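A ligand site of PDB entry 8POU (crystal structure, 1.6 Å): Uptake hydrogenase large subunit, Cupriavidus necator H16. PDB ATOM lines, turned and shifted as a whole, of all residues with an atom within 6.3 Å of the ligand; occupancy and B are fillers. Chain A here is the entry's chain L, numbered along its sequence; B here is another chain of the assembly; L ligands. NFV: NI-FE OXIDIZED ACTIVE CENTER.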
ATOM      1  N   GLU A  27      -2.651 -22.845  20.765  1.00  0.00           N
ATOM      2  CA  GLU A  27      -2.934 -23.975  19.907  1.00  0.00           C
ATOM      3  C   GLU A  27      -2.195 -25.179  20.477  1.00  0.00           C
ATOM      4  O   GLU A  27      -1.000 -25.111  20.765  1.00  0.00           O
ATOM      5  CB  GLU A  27      -2.489 -23.715  18.467  1.00  0.00           C
ATOM      6  CG  GLU A  27      -2.909 -24.798  17.463  1.00  0.00           C
ATOM      7  CD  GLU A  27      -2.310 -26.185  17.743  1.00  0.00           C
ATOM      8  OE1 GLU A  27      -1.119 -26.260  18.145  1.00  0.00           O
ATOM      9  OE2 GLU A  27      -3.029 -27.199  17.572  1.00  0.00           O
ATOM     10  N   ILE A  74      -0.188 -30.009   9.780  1.00  0.00           N
ATOM     11  CA  ILE A  74       0.548 -29.731  11.014  1.00  0.00           C
ATOM     12  C   ILE A  74      -0.262 -28.747  11.857  1.00  0.00           C
ATOM     13  O   ILE A  74      -0.342 -28.886  13.076  1.00  0.00           O
ATOM     14  CB  ILE A  74       1.978 -29.177  10.724  1.00  0.00           C
ATOM     15  CG1 ILE A  74       2.847 -30.324  10.213  1.00  0.00           C
ATOM     16  CG2 ILE A  74       2.638 -28.550  11.966  1.00  0.00           C
ATOM     17  CD1 ILE A  74       4.171 -29.865   9.627  1.00  0.00           C
ATOM     18  N   CYS A  75      -0.902 -27.775  11.217  1.00  0.00           N
ATOM     19  CA  CYS A  75      -1.599 -26.724  11.972  1.00  0.00           C
ATOM     20  C   CYS A  75      -2.681 -25.994  11.188  1.00  0.00           C
ATOM     21  O   CYS A  75      -2.437 -25.496  10.108  1.00  0.00           O
ATOM     22  CB  CYS A  75      -0.578 -25.712  12.424  1.00  0.00           C
ATOM     23  SG  CYS A  75      -1.306 -24.537  13.580  1.00  0.00           S
ATOM     24  N   GLY A  76      -3.877 -25.910  11.783  1.00  0.00           N
ATOM     25  CA  GLY A  76      -4.986 -25.195  11.173  1.00  0.00           C
ATOM     26  C   GLY A  76      -5.118 -23.757  11.614  1.00  0.00           C
ATOM     27  O   GLY A  76      -6.012 -23.058  11.140  1.00  0.00           O
ATOM     28  N   VAL A  77      -4.231 -23.316  12.507  1.00  0.00           N
ATOM     29  CA  VAL A  77      -4.176 -21.924  12.940  1.00  0.00           C
ATOM     30  C   VAL A  77      -3.266 -21.179  11.978  1.00  0.00           C
ATOM     31  O   VAL A  77      -3.693 -20.237  11.320  1.00  0.00           O
ATOM     32  CB  VAL A  77      -3.667 -21.818  14.399  1.00  0.00           C
ATOM     33  CG1 VAL A  77      -3.595 -20.360  14.829  1.00  0.00           C
ATOM     34  CG2 VAL A  77      -4.592 -22.599  15.336  1.00  0.00           C
ATOM     35  N   CYS A  78      -2.012 -21.610  11.863  1.00  0.00           N
ATOM     36  CA  CYS A  78      -1.106 -21.040  10.856  1.00  0.00           C
ATOM     37  C   CYS A  78      -1.328 -21.800   9.542  1.00  0.00           C
ATOM     38  O   CYS A  78      -0.391 -22.314   8.910  1.00  0.00           O
ATOM     39  CB  CYS A  78       0.349 -21.050  11.321  1.00  0.00           C
ATOM     40  SG  CYS A  78       1.003 -22.655  11.804  1.00  0.00           S
ATOM     41  N   THR A  79      -2.595 -21.846   9.135  1.00  0.00           N
ATOM     42  CA  THR A  79      -3.009 -22.703   8.014  1.00  0.00           C
ATOM     43  C   THR A  79      -2.478 -22.182   6.669  1.00  0.00           C
ATOM     44  O   THR A  79      -2.721 -21.029   6.286  1.00  0.00           O
ATOM     45  CB  THR A  79      -4.550 -22.900   7.982  1.00  0.00           C
ATOM     46  OG1 THR A  79      -4.902 -23.753   6.899  1.00  0.00           O
ATOM     47  CG2 THR A  79      -5.330 -21.562   7.844  1.00  0.00           C
ATOM     48  N   CYS A  81       0.843 -21.888   5.877  1.00  0.00           N
ATOM     49  CA  CYS A  81       2.275 -21.563   5.909  1.00  0.00           C
ATOM     50  C   CYS A  81       3.166 -22.790   5.691  1.00  0.00           C
ATOM     51  O   CYS A  81       4.222 -22.685   5.060  1.00  0.00           O
ATOM     52  CB  CYS A  81       2.671 -20.776   7.149  1.00  0.00           C
ATOM     53  SG  CYS A  81       2.768 -21.720   8.661  1.00  0.00           S
ATOM     54  N   HIS A  82       2.753 -23.939   6.194  1.00  0.00           N
ATOM     55  CA  HIS A  82       3.458 -25.194   5.952  1.00  0.00           C
ATOM     56  C   HIS A  82       3.338 -25.641   4.505  1.00  0.00           C
ATOM     57  O   HIS A  82       4.274 -26.198   3.944  1.00  0.00           O
ATOM     58  CB  HIS A  82       2.934 -26.293   6.866  1.00  0.00           C
ATOM     59  CG  HIS A  82       3.316 -26.093   8.292  1.00  0.00           C
ATOM     60  ND1 HIS A  82       4.620 -26.181   8.735  1.00  0.00           N
ATOM     61  CD2 HIS A  82       2.580 -25.803   9.385  1.00  0.00           C
ATOM     62  CE1 HIS A  82       4.668 -25.953  10.021  1.00  0.00           C
ATOM     63  NE2 HIS A  82       3.449 -25.722  10.447  1.00  0.00           N
ATOM     64  N   LEU A 113      -2.933 -14.608   6.018  1.00  0.00           N
ATOM     65  CA  LEU A 113      -2.768 -15.470   7.188  1.00  0.00           C
ATOM     66  C   LEU A 113      -2.160 -14.694   8.346  1.00  0.00           C
ATOM     67  O   LEU A 113      -2.611 -14.833   9.472  1.00  0.00           O
ATOM     68  CB  LEU A 113      -1.895 -16.687   6.866  1.00  0.00           C
ATOM     69  CG  LEU A 113      -1.614 -17.610   8.061  1.00  0.00           C
ATOM     70  CD1 LEU A 113      -2.899 -18.263   8.538  1.00  0.00           C
ATOM     71  CD2 LEU A 113      -0.560 -18.670   7.720  1.00  0.00           C
ATOM     72  N   ASP A 117      -4.209 -14.480  11.711  1.00  0.00           N
ATOM     73  CA  ASP A 117      -3.568 -15.160  12.827  1.00  0.00           C
ATOM     74  C   ASP A 117      -3.216 -14.151  13.917  1.00  0.00           C
ATOM     75  O   ASP A 117      -3.555 -14.348  15.085  1.00  0.00           O
ATOM     76  CB  ASP A 117      -2.339 -15.926  12.331  1.00  0.00           C
ATOM     77  CG  ASP A 117      -1.998 -17.119  13.165  1.00  0.00           C
ATOM     78  OD1 ASP A 117      -2.267 -17.125  14.381  1.00  0.00           O
ATOM     79  OD2 ASP A 117      -1.442 -18.088  12.578  1.00  0.00           O
ATOM     80  N   ALA A 528       6.641 -17.312   8.906  1.00  0.00           N
ATOM     81  CA  ALA A 528       5.347 -17.686   9.429  1.00  0.00           C
ATOM     82  C   ALA A 528       4.923 -16.728  10.549  1.00  0.00           C
ATOM     83  O   ALA A 528       5.770 -16.009  11.085  1.00  0.00           O
ATOM     84  CB  ALA A 528       5.399 -19.108   9.946  1.00  0.00           C
ATOM     85  N   PRO A 529       3.612 -16.684  10.879  1.00  0.00           N
ATOM     86  CA  PRO A 529       3.145 -15.741  11.901  1.00  0.00           C
ATOM     87  C   PRO A 529       3.974 -15.744  13.219  1.00  0.00           C
ATOM     88  O   PRO A 529       4.206 -14.686  13.792  1.00  0.00           O
ATOM     89  CB  PRO A 529       1.701 -16.169  12.128  1.00  0.00           C
ATOM     90  CG  PRO A 529       1.264 -16.652  10.782  1.00  0.00           C
ATOM     91  CD  PRO A 529       2.480 -17.348  10.196  1.00  0.00           C
ATOM     92  N   ARG A 530       4.434 -16.924  13.641  1.00  0.00           N
ATOM     93  CA  ARG A 530       5.158 -17.076  14.904  1.00  0.00           C
ATOM     94  C   ARG A 530       6.683 -17.013  14.791  1.00  0.00           C
ATOM     95  O   ARG A 530       7.387 -17.046  15.805  1.00  0.00           O
ATOM     96  CB  ARG A 530       4.705 -18.369  15.587  1.00  0.00           C
ATOM     97  CG  ARG A 530       3.288 -18.249  16.113  1.00  0.00           C
ATOM     98  CD  ARG A 530       2.597 -19.591  16.222  1.00  0.00           C
ATOM     99  NE  ARG A 530       1.194 -19.351  16.574  1.00  0.00           N
ATOM    100  CZ  ARG A 530       0.229 -19.077  15.696  1.00  0.00           C
ATOM    101  NH1 ARG A 530       0.447 -19.035  14.388  1.00  0.00           N
ATOM    102  NH2 ARG A 530      -0.986 -18.846  16.154  1.00  0.00           N
ATOM    103  N   GLY A 531       7.223 -16.901  13.575  1.00  0.00           N
ATOM    104  CA  GLY A 531       8.666 -16.745  13.380  1.00  0.00           C
ATOM    105  C   GLY A 531       9.191 -17.505  12.189  1.00  0.00           C
ATOM    106  O   GLY A 531       8.499 -17.670  11.173  1.00  0.00           O
ATOM    107  N   ALA A 532      10.414 -18.018  12.327  1.00  0.00           N
ATOM    108  CA  ALA A 532      11.136 -18.652  11.253  1.00  0.00           C
ATOM    109  C   ALA A 532      10.735 -20.118  11.032  1.00  0.00           C
ATOM    110  O   ALA A 532      10.933 -20.965  11.897  1.00  0.00           O
ATOM    111  CB  ALA A 532      12.628 -18.550  11.541  1.00  0.00           C
ATOM    112  N   LEU A 533      10.165 -20.394   9.862  1.00  0.00           N
ATOM    113  CA  LEU A 533       9.751 -21.737   9.483  1.00  0.00           C
ATOM    114  C   LEU A 533      10.613 -22.258   8.353  1.00  0.00           C
ATOM    115  O   LEU A 533      10.843 -21.541   7.375  1.00  0.00           O
ATOM    116  CB  LEU A 533       8.293 -21.741   9.028  1.00  0.00           C
ATOM    117  CG  LEU A 533       7.796 -23.022   8.361  1.00  0.00           C
ATOM    118  CD1 LEU A 533       7.837 -24.228   9.293  1.00  0.00           C
ATOM    119  CD2 LEU A 533       6.399 -22.817   7.824  1.00  0.00           C
ATOM    120  N   HIS A 535      11.259 -26.071   5.937  1.00  0.00           N
ATOM    121  CA  HIS A 535      11.079 -27.479   5.590  1.00  0.00           C
ATOM    122  C   HIS A 535      12.252 -27.886   4.745  1.00  0.00           C
ATOM    123  O   HIS A 535      12.571 -27.214   3.765  1.00  0.00           O
ATOM    124  CB  HIS A 535       9.821 -27.715   4.754  1.00  0.00           C
ATOM    125  CG  HIS A 535       8.542 -27.548   5.498  1.00  0.00           C
ATOM    126  ND1 HIS A 535       7.347 -28.057   5.043  1.00  0.00           N
ATOM    127  CD2 HIS A 535       8.268 -26.906   6.661  1.00  0.00           C
ATOM    128  CE1 HIS A 535       6.391 -27.741   5.899  1.00  0.00           C
ATOM    129  NE2 HIS A 535       6.921 -27.032   6.883  1.00  0.00           N
ATOM    130  N   VAL A 551      10.131 -25.499  13.061  1.00  0.00           N
ATOM    131  CA  VAL A 551       8.985 -24.611  13.055  1.00  0.00           C
ATOM    132  C   VAL A 551       9.199 -23.483  14.101  1.00  0.00           C
ATOM    133  O   VAL A 551       9.951 -23.676  15.068  1.00  0.00           O
ATOM    134  CB  VAL A 551       7.748 -25.519  13.319  1.00  0.00           C
ATOM    135  CG1 VAL A 551       6.450 -24.785  13.131  1.00  0.00           C
ATOM    136  CG2 VAL A 551       7.772 -26.708  12.363  1.00  0.00           C
ATOM    137  N   PRO A 552       8.518 -22.320  13.943  1.00  0.00           N
ATOM    138  CA  PRO A 552       8.827 -21.245  14.877  1.00  0.00           C
ATOM    139  C   PRO A 552       8.695 -21.607  16.355  1.00  0.00           C
ATOM    140  O   PRO A 552       9.587 -21.277  17.134  1.00  0.00           O
ATOM    141  CB  PRO A 552       7.847 -20.138  14.491  1.00  0.00           C
ATOM    142  CG  PRO A 552       7.581 -20.371  13.030  1.00  0.00           C
ATOM    143  CD  PRO A 552       7.643 -21.855  12.848  1.00  0.00           C
ATOM    144  N   THR A 553       7.628 -22.284  16.731  1.00  0.00           N
ATOM    145  CA  THR A 553       7.417 -22.608  18.133  1.00  0.00           C
ATOM    146  C   THR A 553       8.380 -23.731  18.570  1.00  0.00           C
ATOM    147  O   THR A 553       8.634 -23.899  19.765  1.00  0.00           O
ATOM    148  CB  THR A 553       5.928 -22.928  18.437  1.00  0.00           C
ATOM    149  OG1 THR A 553       5.114 -21.820  18.020  1.00  0.00           O
ATOM    150  CG2 THR A 553       5.695 -23.141  19.916  1.00  0.00           C
ATOM    151  N   THR A 554       8.943 -24.476  17.609  1.00  0.00           N
ATOM    152  CA  THR A 554      10.040 -25.410  17.944  1.00  0.00           C
ATOM    153  C   THR A 554      11.213 -24.579  18.510  1.00  0.00           C
ATOM    154  O   THR A 554      11.799 -24.944  19.544  1.00  0.00           O
ATOM    155  CB  THR A 554      10.526 -26.239  16.733  1.00  0.00           C
ATOM    156  OG1 THR A 554       9.416 -26.768  15.994  1.00  0.00           O
ATOM    157  CG2 THR A 554      11.409 -27.381  17.207  1.00  0.00           C
ATOM    158  N   ASP A 595       2.630 -16.367  21.171  1.00  0.00           N
ATOM    159  CA  ASP A 595       1.598 -17.032  20.387  1.00  0.00           C
ATOM    160  C   ASP A 595       1.979 -18.509  20.164  1.00  0.00           C
ATOM    161  O   ASP A 595       2.166 -18.956  19.031  1.00  0.00           O
ATOM    162  CB  ASP A 595       1.441 -16.261  19.071  1.00  0.00           C
ATOM    163  CG  ASP A 595       0.282 -16.721  18.237  1.00  0.00           C
ATOM    164  OD1 ASP A 595      -0.523 -17.561  18.661  1.00  0.00           O
ATOM    165  OD2 ASP A 595       0.203 -16.220  17.097  1.00  0.00           O
ATOM    166  N   PRO A 596       2.107 -19.284  21.250  1.00  0.00           N
ATOM    167  CA  PRO A 596       2.560 -20.668  21.084  1.00  0.00           C
ATOM    168  C   PRO A 596       1.629 -21.524  20.229  1.00  0.00           C
ATOM    169  O   PRO A 596       0.413 -21.542  20.445  1.00  0.00           O
ATOM    170  CB  PRO A 596       2.599 -21.196  22.530  1.00  0.00           C
ATOM    171  CG  PRO A 596       2.681 -19.978  23.390  1.00  0.00           C
ATOM    172  CD  PRO A 596       1.885 -18.949  22.663  1.00  0.00           C
ATOM    173  N   CYS A 597       2.193 -22.226  19.267  1.00  0.00           N
ATOM    174  CA  CYS A 597       1.470 -23.235  18.516  1.00  0.00           C
ATOM    175  C   CYS A 597       2.149 -24.565  18.733  1.00  0.00           C
ATOM    176  O   CYS A 597       3.191 -24.859  18.164  1.00  0.00           O
ATOM    177  CB  CYS A 597       1.409 -22.884  17.057  1.00  0.00           C
ATOM    178  SG  CYS A 597       0.290 -23.972  16.123  1.00  0.00           S
ATOM    179  N   LEU A 598       1.551 -25.384  19.578  1.00  0.00           N
ATOM    180  CA  LEU A 598       2.232 -26.577  20.030  1.00  0.00           C
ATOM    181  C   LEU A 598       2.169 -27.688  19.002  1.00  0.00           C
ATOM    182  O   LEU A 598       3.076 -28.502  18.946  1.00  0.00           O
ATOM    183  CB  LEU A 598       1.718 -27.029  21.397  1.00  0.00           C
ATOM    184  CG  LEU A 598       2.377 -26.271  22.558  1.00  0.00           C
ATOM    185  CD1 LEU A 598       3.786 -26.774  22.808  1.00  0.00           C
ATOM    186  CD2 LEU A 598       2.413 -24.747  22.371  1.00  0.00           C
ATOM    187  N   ALA A 599       1.110 -27.714  18.186  1.00  0.00           N
ATOM    188  CA  ALA A 599       1.008 -28.713  17.127  1.00  0.00           C
ATOM    189  C   ALA A 599       2.102 -28.432  16.115  1.00  0.00           C
ATOM    190  O   ALA A 599       2.752 -29.362  15.628  1.00  0.00           O
ATOM    191  CB  ALA A 599      -0.361 -28.694  16.490  1.00  0.00           C
ATOM    192  N   CYS A 600       2.292 -27.150  15.802  1.00  0.00           N
ATOM    193  CA  CYS A 600       3.427 -26.720  14.995  1.00  0.00           C
ATOM    194  C   CYS A 600       4.756 -27.149  15.589  1.00  0.00           C
ATOM    195  O   CYS A 600       5.595 -27.713  14.891  1.00  0.00           O
ATOM    196  CB  CYS A 600       3.428 -25.202  14.850  1.00  0.00           C
ATOM    197  SG  CYS A 600       2.572 -24.658  13.380  1.00  0.00           S
ATOM    198  N   SER A 601       4.970 -26.854  16.874  1.00  0.00           N
ATOM    199  CA  SER A 601       6.270 -27.085  17.502  1.00  0.00           C
ATOM    200  C   SER A 601       6.751 -28.532  17.409  1.00  0.00           C
ATOM    201  O   SER A 601       7.941 -28.778  17.322  1.00  0.00           O
ATOM    202  CB  SER A 601       6.264 -26.635  18.971  1.00  0.00           C
ATOM    203  OG  SER A 601       5.547 -27.539  19.786  1.00  0.00           O
ATOM    204  N   CYS B  17      -4.819 -30.498  14.747  1.00  0.00           N
ATOM    205  CA  CYS B  17      -4.168 -29.292  14.225  1.00  0.00           C
ATOM    206  C   CYS B  17      -4.929 -28.012  14.575  1.00  0.00           C
ATOM    207  O   CYS B  17      -4.451 -26.923  14.277  1.00  0.00           O
ATOM    208  CB  CYS B  17      -4.008 -29.413  12.717  1.00  0.00           C
ATOM    209  SG  CYS B  17      -5.431 -28.887  11.757  1.00  0.00           S
HETATM  210 FE   NFV L   1       2.974 -22.341  13.038  1.00  0.00          FE
HETATM  211 NI   NFV L   1       0.449 -23.272  14.081  1.00  0.00          NI
HETATM  212  C1  NFV L   1       4.220 -22.601  11.749  1.00  0.00           C
HETATM  213  O1  NFV L   1       5.016 -22.775  10.936  1.00  0.00           O
HETATM  214  C2  NFV L   1       4.301 -22.246  14.406  1.00  0.00           C
HETATM  215  N2  NFV L   1       5.076 -22.202  15.228  1.00  0.00           N
HETATM  216  C3  NFV L   1       3.195 -20.472  12.741  1.00  0.00           C
HETATM  217  N3  NFV L   1       3.319 -19.396  12.595  1.00  0.00           N
HETATM  218  O4  NFV L   1       1.571 -21.879  14.618  1.00  0.00           O
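A nitrogen (N3) of the ligand sits close to the backbone nitrogen (N) of Pro 529 (3.2 Å).
Merely in contact with the ligand: Ala 528 (3.4 Å), Leu 533 (3.4 Å), Val 551 (3.3 Å) and Pro 552 (3.4 Å).
Hydrophobic or aromatic side chains within 4 Å of the ligand: His 82, Ala 528, Pro 529, Leu 533, Val 551 and Pro 552.
The nearest printed residue that does not touch the ligand is Val 77 (4.4 Å).
SG of Cys 597 is bound to NI of the ligand, at 2.2 Å.
NI of the ligand is bound by SG of Cys 75.
The side-chain sulfur (SG) of Cys 78 binds an iron atom (FE) of the ligand (2.3 Å).
FE of the ligand is bound by SG of Cys 600, at 2.4 Å.
N2 of the ligand lies within hydrogen-bond range of N of Thr 553.
The side-chain hydroxyl of Thr 553 is in hydrogen-bond range of a nitrogen (N2) of the ligand, at 2.8 Å.
The backbone NH (N) of Arg 530 sits at hydrogen-bond distance from a nitrogen (N3) of the ligand (2.9 Å).
The guanidinium group (NH1) of Arg 530 is in hydrogen-bond range of a nitrogen (N3) of the ligand.
NE2 of His 82 lies close to O1 of the ligand, 3.4 Å away.
SG of Cys 81 is in hydrogen-bond range of O1 of the ligand (3.4 Å).
N of Cys 597 sits at hydrogen-bond distance from OG1 of Thr 553 (3.2 Å).
OE1 of Glu 27 sits close to SG of Cys 597, 3.4 Å away.
N of Val 77 sits close to SG of Cys 75, 3.3 Å away.
The backbone carbonyl oxygen (O) of Cys 78 lies within hydrogen-bond range of the side-chain sulfur (SG) of Cys 81 (3.2 Å).
A ring nitrogen (NE2) of His 82 sits close to the side-chain sulfur (SG) of Cys 600 (3.2 Å).
The guanidinium group of Arg 530 is in salt-bridge range of the side-chain carboxylate of Asp 117 (2.8 Å).
The guanidinium group (NH2) of Arg 530 lies within salt-bridge range of the side-chain carboxylate (OD1) of Asp 595.
The side-chain hydroxyl of Thr 554 sits close to the backbone carbonyl oxygen of Val 551 (3.3 Å).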
